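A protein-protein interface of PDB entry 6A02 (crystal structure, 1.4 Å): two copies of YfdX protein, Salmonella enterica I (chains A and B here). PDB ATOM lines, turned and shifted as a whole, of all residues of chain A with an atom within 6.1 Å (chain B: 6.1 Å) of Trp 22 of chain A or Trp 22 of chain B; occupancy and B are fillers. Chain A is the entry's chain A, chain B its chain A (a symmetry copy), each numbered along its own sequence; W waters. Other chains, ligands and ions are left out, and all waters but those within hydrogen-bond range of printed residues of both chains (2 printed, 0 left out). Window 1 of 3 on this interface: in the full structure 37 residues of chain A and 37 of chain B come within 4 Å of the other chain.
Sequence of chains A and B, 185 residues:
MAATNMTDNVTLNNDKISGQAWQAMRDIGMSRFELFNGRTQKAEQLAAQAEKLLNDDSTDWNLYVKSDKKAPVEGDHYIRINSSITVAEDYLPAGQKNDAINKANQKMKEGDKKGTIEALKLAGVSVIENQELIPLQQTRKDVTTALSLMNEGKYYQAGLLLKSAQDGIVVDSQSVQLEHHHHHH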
ATOM      1  N   SER A  18      -0.163  21.453   1.485  1.00  0.00           N
ATOM      2  CA  SER A  18       0.217  22.817   1.110  1.00  0.00           C
ATOM      3  C   SER A  18       0.787  23.570   2.307  1.00  0.00           C
ATOM      4  O   SER A  18       0.041  24.027   3.180  1.00  0.00           O
ATOM      5  CB  SER A  18      -0.948  23.591   0.503  1.00  0.00           C
ATOM      6  OG  SER A  18      -0.563  24.944   0.290  1.00  0.00           O
ATOM      7  N   GLY A  19       2.107  23.752   2.321  1.00  0.00           N
ATOM      8  CA  GLY A  19       2.698  24.595   3.343  1.00  0.00           C
ATOM      9  C   GLY A  19       2.346  26.058   3.183  1.00  0.00           C
ATOM     10  O   GLY A  19       2.281  26.793   4.174  1.00  0.00           O
ATOM     11  N   GLN A  20       2.127  26.505   1.941  1.00  0.00           N
ATOM     12  CA  GLN A  20       1.720  27.889   1.725  1.00  0.00           C
ATOM     13  C   GLN A  20       0.351  28.155   2.334  1.00  0.00           C
ATOM     14  O   GLN A  20       0.140  29.195   2.970  1.00  0.00           O
ATOM     15  CB  GLN A  20       1.684  28.219   0.237  1.00  0.00           C
ATOM     16  CG  GLN A  20       3.044  28.340  -0.429  1.00  0.00           C
ATOM     17  CD  GLN A  20       2.904  28.526  -1.921  1.00  0.00           C
ATOM     18  OE1 GLN A  20       2.298  27.697  -2.603  1.00  0.00           O
ATOM     19  NE2 GLN A  20       3.444  29.628  -2.439  1.00  0.00           N
ATOM     20  N   ALA A  21      -0.595  27.237   2.135  1.00  0.00           N
ATOM     21  CA  ALA A  21      -1.929  27.441   2.690  1.00  0.00           C
ATOM     22  C   ALA A  21      -1.923  27.322   4.204  1.00  0.00           C
ATOM     23  O   ALA A  21      -2.701  28.005   4.882  1.00  0.00           O
ATOM     24  CB  ALA A  21      -2.919  26.454   2.080  1.00  0.00           C
ATOM     25  N   TRP A  22      -1.076  26.453   4.758  1.00  0.00           N
ATOM     26  CA  TRP A  22      -0.936  26.428   6.208  1.00  0.00           C
ATOM     27  C   TRP A  22      -0.479  27.783   6.731  1.00  0.00           C
ATOM     28  O   TRP A  22      -1.054  28.315   7.689  1.00  0.00           O
ATOM     29  CB  TRP A  22       0.019  25.308   6.642  1.00  0.00           C
ATOM     30  CG  TRP A  22      -0.060  25.087   8.111  1.00  0.00           C
ATOM     31  CD1 TRP A  22      -0.929  24.270   8.773  1.00  0.00           C
ATOM     32  CD2 TRP A  22       0.729  25.728   9.105  1.00  0.00           C
ATOM     33  NE1 TRP A  22      -0.719  24.353  10.128  1.00  0.00           N
ATOM     34  CE2 TRP A  22       0.303  25.239  10.354  1.00  0.00           C
ATOM     35  CE3 TRP A  22       1.770  26.655   9.059  1.00  0.00           C
ATOM     36  CZ2 TRP A  22       0.869  25.657  11.549  1.00  0.00           C
ATOM     37  CZ3 TRP A  22       2.336  27.067  10.246  1.00  0.00           C
ATOM     38  CH2 TRP A  22       1.886  26.564  11.472  1.00  0.00           C
ATOM     39  N   GLN A  23       0.549  28.364   6.106  1.00  0.00           N
ATOM     40  CA  GLN A  23       1.037  29.663   6.552  1.00  0.00           C
ATOM     41  C   GLN A  23      -0.008  30.747   6.336  1.00  0.00           C
ATOM     42  O   GLN A  23      -0.106  31.680   7.140  1.00  0.00           O
ATOM     43  CB  GLN A  23       2.339  30.001   5.827  1.00  0.00           C
ATOM     44  CG  GLN A  23       2.990  31.299   6.304  1.00  0.00           C
ATOM     45  CD  GLN A  23       3.403  31.219   7.755  1.00  0.00           C
ATOM     46  OE1 GLN A  23       3.979  30.221   8.186  1.00  0.00           O
ATOM     47  NE2 GLN A  23       3.072  32.252   8.531  1.00  0.00           N
ATOM     48  N   ALA A  24      -0.802  30.628   5.273  1.00  0.00           N
ATOM     49  CA  ALA A  24      -1.873  31.589   5.039  1.00  0.00           C
ATOM     50  C   ALA A  24      -2.877  31.570   6.183  1.00  0.00           C
ATOM     51  O   ALA A  24      -3.323  32.628   6.645  1.00  0.00           O
ATOM     52  CB  ALA A  24      -2.567  31.289   3.708  1.00  0.00           C
ATOM     53  N   MET A  25      -3.228  30.377   6.671  1.00  0.00           N
ATOM     54  CA  MET A  25      -4.174  30.307   7.782  1.00  0.00           C
ATOM     55  C   MET A  25      -3.573  30.899   9.048  1.00  0.00           C
ATOM     56  O   MET A  25      -4.277  31.555   9.825  1.00  0.00           O
ATOM     57  CB  MET A  25      -4.609  28.859   8.015  1.00  0.00           C
ATOM     58  CG  MET A  25      -5.371  28.236   6.847  1.00  0.00           C
ATOM     59  SD  MET A  25      -6.686  29.286   6.188  1.00  0.00           S
ATOM     60  CE  MET A  25      -7.745  29.420   7.623  1.00  0.00           C
ATOM     61  N   ARG A  26      -2.277  30.675   9.272  1.00  0.00           N
ATOM     62  CA  ARG A  26      -1.594  31.304  10.396  1.00  0.00           C
ATOM     63  C   ARG A  26      -1.645  32.824  10.264  1.00  0.00           C
ATOM     64  O   ARG A  26      -1.961  33.539  11.228  1.00  0.00           O
ATOM     65  CB  ARG A  26      -0.163  30.764  10.441  1.00  0.00           C
ATOM     66  CG  ARG A  26       0.833  31.559  11.238  1.00  0.00           C
ATOM     67  CD  ARG A  26       0.476  31.670  12.692  1.00  0.00           C
ATOM     68  NE  ARG A  26       1.625  32.174  13.444  1.00  0.00           N
ATOM     69  CZ  ARG A  26       1.567  32.592  14.704  1.00  0.00           C
ATOM     70  NH1 ARG A  26       0.415  32.581  15.346  1.00  0.00           N
ATOM     71  NH2 ARG A  26       2.665  33.031  15.311  1.00  0.00           N
ATOM     72  N   ASP A  27      -1.397  33.335   9.052  1.00  0.00           N
ATOM     73  CA  ASP A  27      -1.442  34.779   8.826  1.00  0.00           C
ATOM     74  C   ASP A  27      -2.846  35.341   9.047  1.00  0.00           C
ATOM     75  O   ASP A  27      -2.997  36.461   9.555  1.00  0.00           O
ATOM     76  CB  ASP A  27      -0.970  35.103   7.407  1.00  0.00           C
ATOM     77  CG  ASP A  27       0.515  34.874   7.203  1.00  0.00           C
ATOM     78  OD1 ASP A  27       1.240  34.639   8.199  1.00  0.00           O
ATOM     79  OD2 ASP A  27       0.941  34.945   6.027  1.00  0.00           O
ATOM     80  N   ILE A  81      -3.768  20.963   4.358  1.00  0.00           N
ATOM     81  CA  ILE A  81      -2.818  21.926   4.903  1.00  0.00           C
ATOM     82  C   ILE A  81      -1.977  21.385   6.049  1.00  0.00           C
ATOM     83  O   ILE A  81      -0.980  22.027   6.412  1.00  0.00           O
ATOM     84  CB  ILE A  81      -3.474  23.274   5.292  1.00  0.00           C
ATOM     85  CG1 ILE A  81      -4.330  23.132   6.553  1.00  0.00           C
ATOM     86  CG2 ILE A  81      -4.283  23.820   4.136  1.00  0.00           C
ATOM     87  CD1 ILE A  81      -4.817  24.465   7.109  1.00  0.00           C
ATOM     88  N   ASN A  82      -2.330  20.242   6.629  1.00  0.00           N
ATOM     89  CA  ASN A  82      -1.510  19.659   7.685  1.00  0.00           C
ATOM     90  C   ASN A  82      -1.912  18.207   7.857  1.00  0.00           C
ATOM     91  O   ASN A  82      -3.042  17.822   7.551  1.00  0.00           O
ATOM     92  CB  ASN A  82      -1.666  20.418   9.010  1.00  0.00           C
ATOM     93  CG  ASN A  82      -0.636  20.002  10.036  1.00  0.00           C
ATOM     94  OD1 ASN A  82       0.549  20.206   9.837  1.00  0.00           O
ATOM     95  ND2 ASN A  82      -1.086  19.397  11.133  1.00  0.00           N
ATOM     96  N   GLU A 132      -5.840  18.114   8.219  1.00  0.00           N
ATOM     97  CA  GLU A 132      -6.470  19.419   8.307  1.00  0.00           C
ATOM     98  C   GLU A 132      -6.687  19.936   6.893  1.00  0.00           C
ATOM     99  O   GLU A 132      -5.755  19.940   6.085  1.00  0.00           O
ATOM    100  CB  GLU A 132      -5.556  20.362   9.084  1.00  0.00           C
ATOM    101  CG  GLU A 132      -6.166  21.709   9.346  1.00  0.00           C
ATOM    102  CD  GLU A 132      -5.233  22.668  10.078  1.00  0.00           C
ATOM    103  OE1 GLU A 132      -4.081  22.291  10.364  1.00  0.00           O
ATOM    104  OE2 GLU A 132      -5.663  23.809  10.366  1.00  0.00           O
ATOM    105  N   SER B  18       6.429  34.971  22.148  1.00  0.00           N
ATOM    106  CA  SER B  18       7.609  34.362  21.531  1.00  0.00           C
ATOM    107  C   SER B  18       7.252  33.713  20.200  1.00  0.00           C
ATOM    108  O   SER B  18       6.679  32.617  20.164  1.00  0.00           O
ATOM    109  CB  SER B  18       8.280  33.350  22.452  1.00  0.00           C
ATOM    110  OG  SER B  18       9.330  32.691  21.753  1.00  0.00           O
ATOM    111  N   GLY B  19       7.639  34.357  19.099  1.00  0.00           N
ATOM    112  CA  GLY B  19       7.476  33.720  17.807  1.00  0.00           C
ATOM    113  C   GLY B  19       8.386  32.528  17.611  1.00  0.00           C
ATOM    114  O   GLY B  19       8.038  31.592  16.884  1.00  0.00           O
ATOM    115  N   GLN B  20       9.566  32.545  18.244  1.00  0.00           N
ATOM    116  CA  GLN B  20      10.461  31.397  18.149  1.00  0.00           C
ATOM    117  C   GLN B  20       9.842  30.171  18.803  1.00  0.00           C
ATOM    118  O   GLN B  20       9.916  29.064  18.254  1.00  0.00           O
ATOM    119  CB  GLN B  20      11.803  31.699  18.807  1.00  0.00           C
ATOM    120  CG  GLN B  20      12.691  32.667  18.044  1.00  0.00           C
ATOM    121  CD  GLN B  20      13.928  33.011  18.839  1.00  0.00           C
ATOM    122  OE1 GLN B  20      13.834  33.501  19.966  1.00  0.00           O
ATOM    123  NE2 GLN B  20      15.101  32.738  18.269  1.00  0.00           N
ATOM    124  N   ALA B  21       9.246  30.341  19.982  1.00  0.00           N
ATOM    125  CA  ALA B  21       8.641  29.201  20.660  1.00  0.00           C
ATOM    126  C   ALA B  21       7.397  28.720  19.934  1.00  0.00           C
ATOM    127  O   ALA B  21       7.102  27.517  19.937  1.00  0.00           O
ATOM    128  CB  ALA B  21       8.312  29.549  22.108  1.00  0.00           C
ATOM    129  N   TRP B  22       6.641  29.633  19.320  1.00  0.00           N
ATOM    130  CA  TRP B  22       5.532  29.189  18.487  1.00  0.00           C
ATOM    131  C   TRP B  22       6.027  28.295  17.358  1.00  0.00           C
ATOM    132  O   TRP B  22       5.471  27.216  17.118  1.00  0.00           O
ATOM    133  CB  TRP B  22       4.745  30.389  17.946  1.00  0.00           C
ATOM    134  CG  TRP B  22       3.456  29.950  17.346  1.00  0.00           C
ATOM    135  CD1 TRP B  22       2.268  29.771  17.991  1.00  0.00           C
ATOM    136  CD2 TRP B  22       3.238  29.584  15.989  1.00  0.00           C
ATOM    137  NE1 TRP B  22       1.312  29.326  17.110  1.00  0.00           N
ATOM    138  CE2 TRP B  22       1.886  29.212  15.870  1.00  0.00           C
ATOM    139  CE3 TRP B  22       4.051  29.555  14.856  1.00  0.00           C
ATOM    140  CZ2 TRP B  22       1.331  28.801  14.668  1.00  0.00           C
ATOM    141  CZ3 TRP B  22       3.499  29.149  13.661  1.00  0.00           C
ATOM    142  CH2 TRP B  22       2.150  28.783  13.577  1.00  0.00           C
ATOM    143  N   GLN B  23       7.083  28.722  16.659  1.00  0.00           N
ATOM    144  CA  GLN B  23       7.611  27.915  15.566  1.00  0.00           C
ATOM    145  C   GLN B  23       8.189  26.605  16.080  1.00  0.00           C
ATOM    146  O   GLN B  23       8.095  25.578  15.399  1.00  0.00           O
ATOM    147  CB  GLN B  23       8.662  28.715  14.796  1.00  0.00           C
ATOM    148  CG  GLN B  23       9.203  27.993  13.563  1.00  0.00           C
ATOM    149  CD  GLN B  23       8.120  27.750  12.537  1.00  0.00           C
ATOM    150  OE1 GLN B  23       7.324  28.640  12.245  1.00  0.00           O
ATOM    151  NE2 GLN B  23       8.055  26.524  12.012  1.00  0.00           N
ATOM    152  N   ALA B  24       8.769  26.619  17.279  1.00  0.00           N
ATOM    153  CA  ALA B  24       9.280  25.389  17.868  1.00  0.00           C
ATOM    154  C   ALA B  24       8.160  24.379  18.075  1.00  0.00           C
ATOM    155  O   ALA B  24       8.328  23.186  17.791  1.00  0.00           O
ATOM    156  CB  ALA B  24       9.982  25.692  19.194  1.00  0.00           C
ATOM    157  N   MET B  25       6.999  24.840  18.547  1.00  0.00           N
ATOM    158  CA  MET B  25       5.886  23.915  18.744  1.00  0.00           C
ATOM    159  C   MET B  25       5.386  23.371  17.415  1.00  0.00           C
ATOM    160  O   MET B  25       5.015  22.195  17.321  1.00  0.00           O
ATOM    161  CB  MET B  25       4.755  24.605  19.509  1.00  0.00           C
ATOM    162  CG  MET B  25       5.124  25.039  20.926  1.00  0.00           C
ATOM    163  SD  MET B  25       5.965  23.758  21.886  1.00  0.00           S
ATOM    164  CE  MET B  25       4.697  22.499  21.930  1.00  0.00           C
ATOM    165  N   ARG B  26       5.366  24.213  16.379  1.00  0.00           N
ATOM    166  CA  ARG B  26       5.017  23.745  15.044  1.00  0.00           C
ATOM    167  C   ARG B  26       6.007  22.679  14.580  1.00  0.00           C
ATOM    168  O   ARG B  26       5.610  21.620  14.068  1.00  0.00           O
ATOM    169  CB  ARG B  26       4.979  24.960  14.113  1.00  0.00           C
ATOM    170  CG  ARG B  26       5.051  24.681  12.639  1.00  0.00           C
ATOM    171  CD  ARG B  26       3.909  23.844  12.136  1.00  0.00           C
ATOM    172  NE  ARG B  26       3.877  23.881  10.674  1.00  0.00           N
ATOM    173  CZ  ARG B  26       3.133  23.076   9.923  1.00  0.00           C
ATOM    174  NH1 ARG B  26       2.374  22.161  10.497  1.00  0.00           N
ATOM    175  NH2 ARG B  26       3.165  23.183   8.601  1.00  0.00           N
ATOM    176  N   ASP B  27       7.303  22.915  14.810  1.00  0.00           N
ATOM    177  CA  ASP B  27       8.321  21.942  14.417  1.00  0.00           C
ATOM    178  C   ASP B  27       8.171  20.629  15.183  1.00  0.00           C
ATOM    179  O   ASP B  27       8.405  19.550  14.623  1.00  0.00           O
ATOM    180  CB  ASP B  27       9.719  22.522  14.648  1.00  0.00           C
ATOM    181  CG  ASP B  27      10.070  23.640  13.685  1.00  0.00           C
ATOM    182  OD1 ASP B  27       9.318  23.862  12.706  1.00  0.00           O
ATOM    183  OD2 ASP B  27      11.119  24.282  13.924  1.00  0.00           O
ATOM    184  N   ILE B  81       3.113  32.114  23.674  1.00  0.00           N
ATOM    185  CA  ILE B  81       3.470  31.782  22.298  1.00  0.00           C
ATOM    186  C   ILE B  81       2.446  32.235  21.268  1.00  0.00           C
ATOM    187  O   ILE B  81       2.764  32.229  20.070  1.00  0.00           O
ATOM    188  CB  ILE B  81       3.818  30.286  22.104  1.00  0.00           C
ATOM    189  CG1 ILE B  81       2.567  29.409  22.182  1.00  0.00           C
ATOM    190  CG2 ILE B  81       4.860  29.852  23.114  1.00  0.00           C
ATOM    191  CD1 ILE B  81       2.816  27.959  21.778  1.00  0.00           C
ATOM    192  N   ASN B  82       1.243  32.624  21.677  1.00  0.00           N
ATOM    193  CA  ASN B  82       0.261  33.129  20.726  1.00  0.00           C
ATOM    194  C   ASN B  82      -0.820  33.864  21.494  1.00  0.00           C
ATOM    195  O   ASN B  82      -1.060  33.587  22.671  1.00  0.00           O
ATOM    196  CB  ASN B  82      -0.355  31.998  19.889  1.00  0.00           C
ATOM    197  CG  ASN B  82      -1.168  32.518  18.726  1.00  0.00           C
ATOM    198  OD1 ASN B  82      -0.632  33.147  17.831  1.00  0.00           O
ATOM    199  ND2 ASN B  82      -2.477  32.273  18.746  1.00  0.00           N
ATOM    200  N   GLU B 132      -2.024  31.475  24.395  1.00  0.00           N
ATOM    201  CA  GLU B 132      -1.460  30.137  24.350  1.00  0.00           C
ATOM    202  C   GLU B 132      -0.106  30.170  25.039  1.00  0.00           C
ATOM    203  O   GLU B 132       0.730  31.022  24.725  1.00  0.00           O
ATOM    204  CB  GLU B 132      -1.304  29.712  22.892  1.00  0.00           C
ATOM    205  CG  GLU B 132      -0.847  28.290  22.726  1.00  0.00           C
ATOM    206  CD  GLU B 132      -0.643  27.883  21.271  1.00  0.00           C
ATOM    207  OE1 GLU B 132      -0.831  28.725  20.374  1.00  0.00           O
ATOM    208  OE2 GLU B 132      -0.286  26.707  21.031  1.00  0.00           O
HETATM  209  O   HOH W   1       1.660  21.507   6.832  1.00  0.00           O
HETATM  210  O   HOH W   2       2.714  34.003  18.003  1.00  0.00           O
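The backbone carbonyl oxygen of Asn 82 of chain B lies within hydrogen-bond range of the backbone NH of Glu 132 of chain B (2.9 Å). The backbone carbonyl oxygen (O) of Asn 82 of chain A is in hydrogen-bond range of the backbone NH (N) of Glu 132 of chain A, 2.9 Å away.
Water W1 lies within hydrogen-bond range of O of Ile 81 of chain A, NH2 of Arg 26 of chain B and OD1 of Asn 82 of chain A. Water W2 lies within hydrogen-bond range of O of Ile 81 of chain B (2.7 Å), NH2 of Arg 26 of chain A (2.9 Å) and OD1 of Asn 82 of chain B (3.5 Å).
OD1 of Asn 82 of chain A lies within hydrogen-bond range of NH1 of Arg 26 of chain B. The guanidinium group (NH1) of Arg 26 of chain A sits at hydrogen-bond distance from the side-chain amide oxygen (OD1) of Asn 82 of chain B (2.8 Å).
Trp 22 of chain A touches just these residues of chain B: Trp 22 and Arg 26. Of chain A, only Trp 22 and Arg 26 come within 4 Å of Trp 22 of chain B. Of the printed residues of chain B, Arg 26 of chain A touches Trp 22 (3.4 Å) and Asn 82 (2.8 Å). Of the printed residues of chain A, Arg 26 of chain B touches Trp 22 and Asn 82. Ala 24 of chain A touches none of the printed residues of chain B. Asp 27 of chain B touches none of the printed residues of chain A. The nearest residue of chain B that does not touch Trp 22 of chain A is Gln 23 of chain B (5.6 Å). The nearest printed residue of chain A that does not touch Arg 26 of chain B is Ile 81 of chain A (4.8 Å).
Of the 13 printed residues of chain B, 3 touch a printed residue of chain A. Hydrophobic or aromatic side chains of chain B within 4 Å of the printed part of chain A: Trp 22. Of the 13 printed residues of chain A, 3 touch a printed residue of chain B. Printed residues of chain A that touch a printed residue of chain B: Trp 22, Arg 26 and Asn 82.
Trp 22 of chain B touches its own counterpart, Trp 22 of chain A. Trp 22 of chain A touches Arg 26 of chain B, and with the chains exchanged Arg 26 of chain A touches Trp 22 of chain B. Arg 26 of chain A touches Asn 82 of chain B, and with the chains exchanged Asn 82 of chain A touches Arg 26 of chain B. Of the 5 pairs that touch across the chains among the printed residues, 5 have their exchanged pair printed and touching as well.
Among the printed residues, merely in contact across the chains: Trp 22 of chain A with Trp 22 of chain B (3.1 Å), Trp 22 of chain A with Arg 26 of chain B (3.4 Å) and Arg 26 of chain A with Trp 22 of chain B (3.4 Å).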
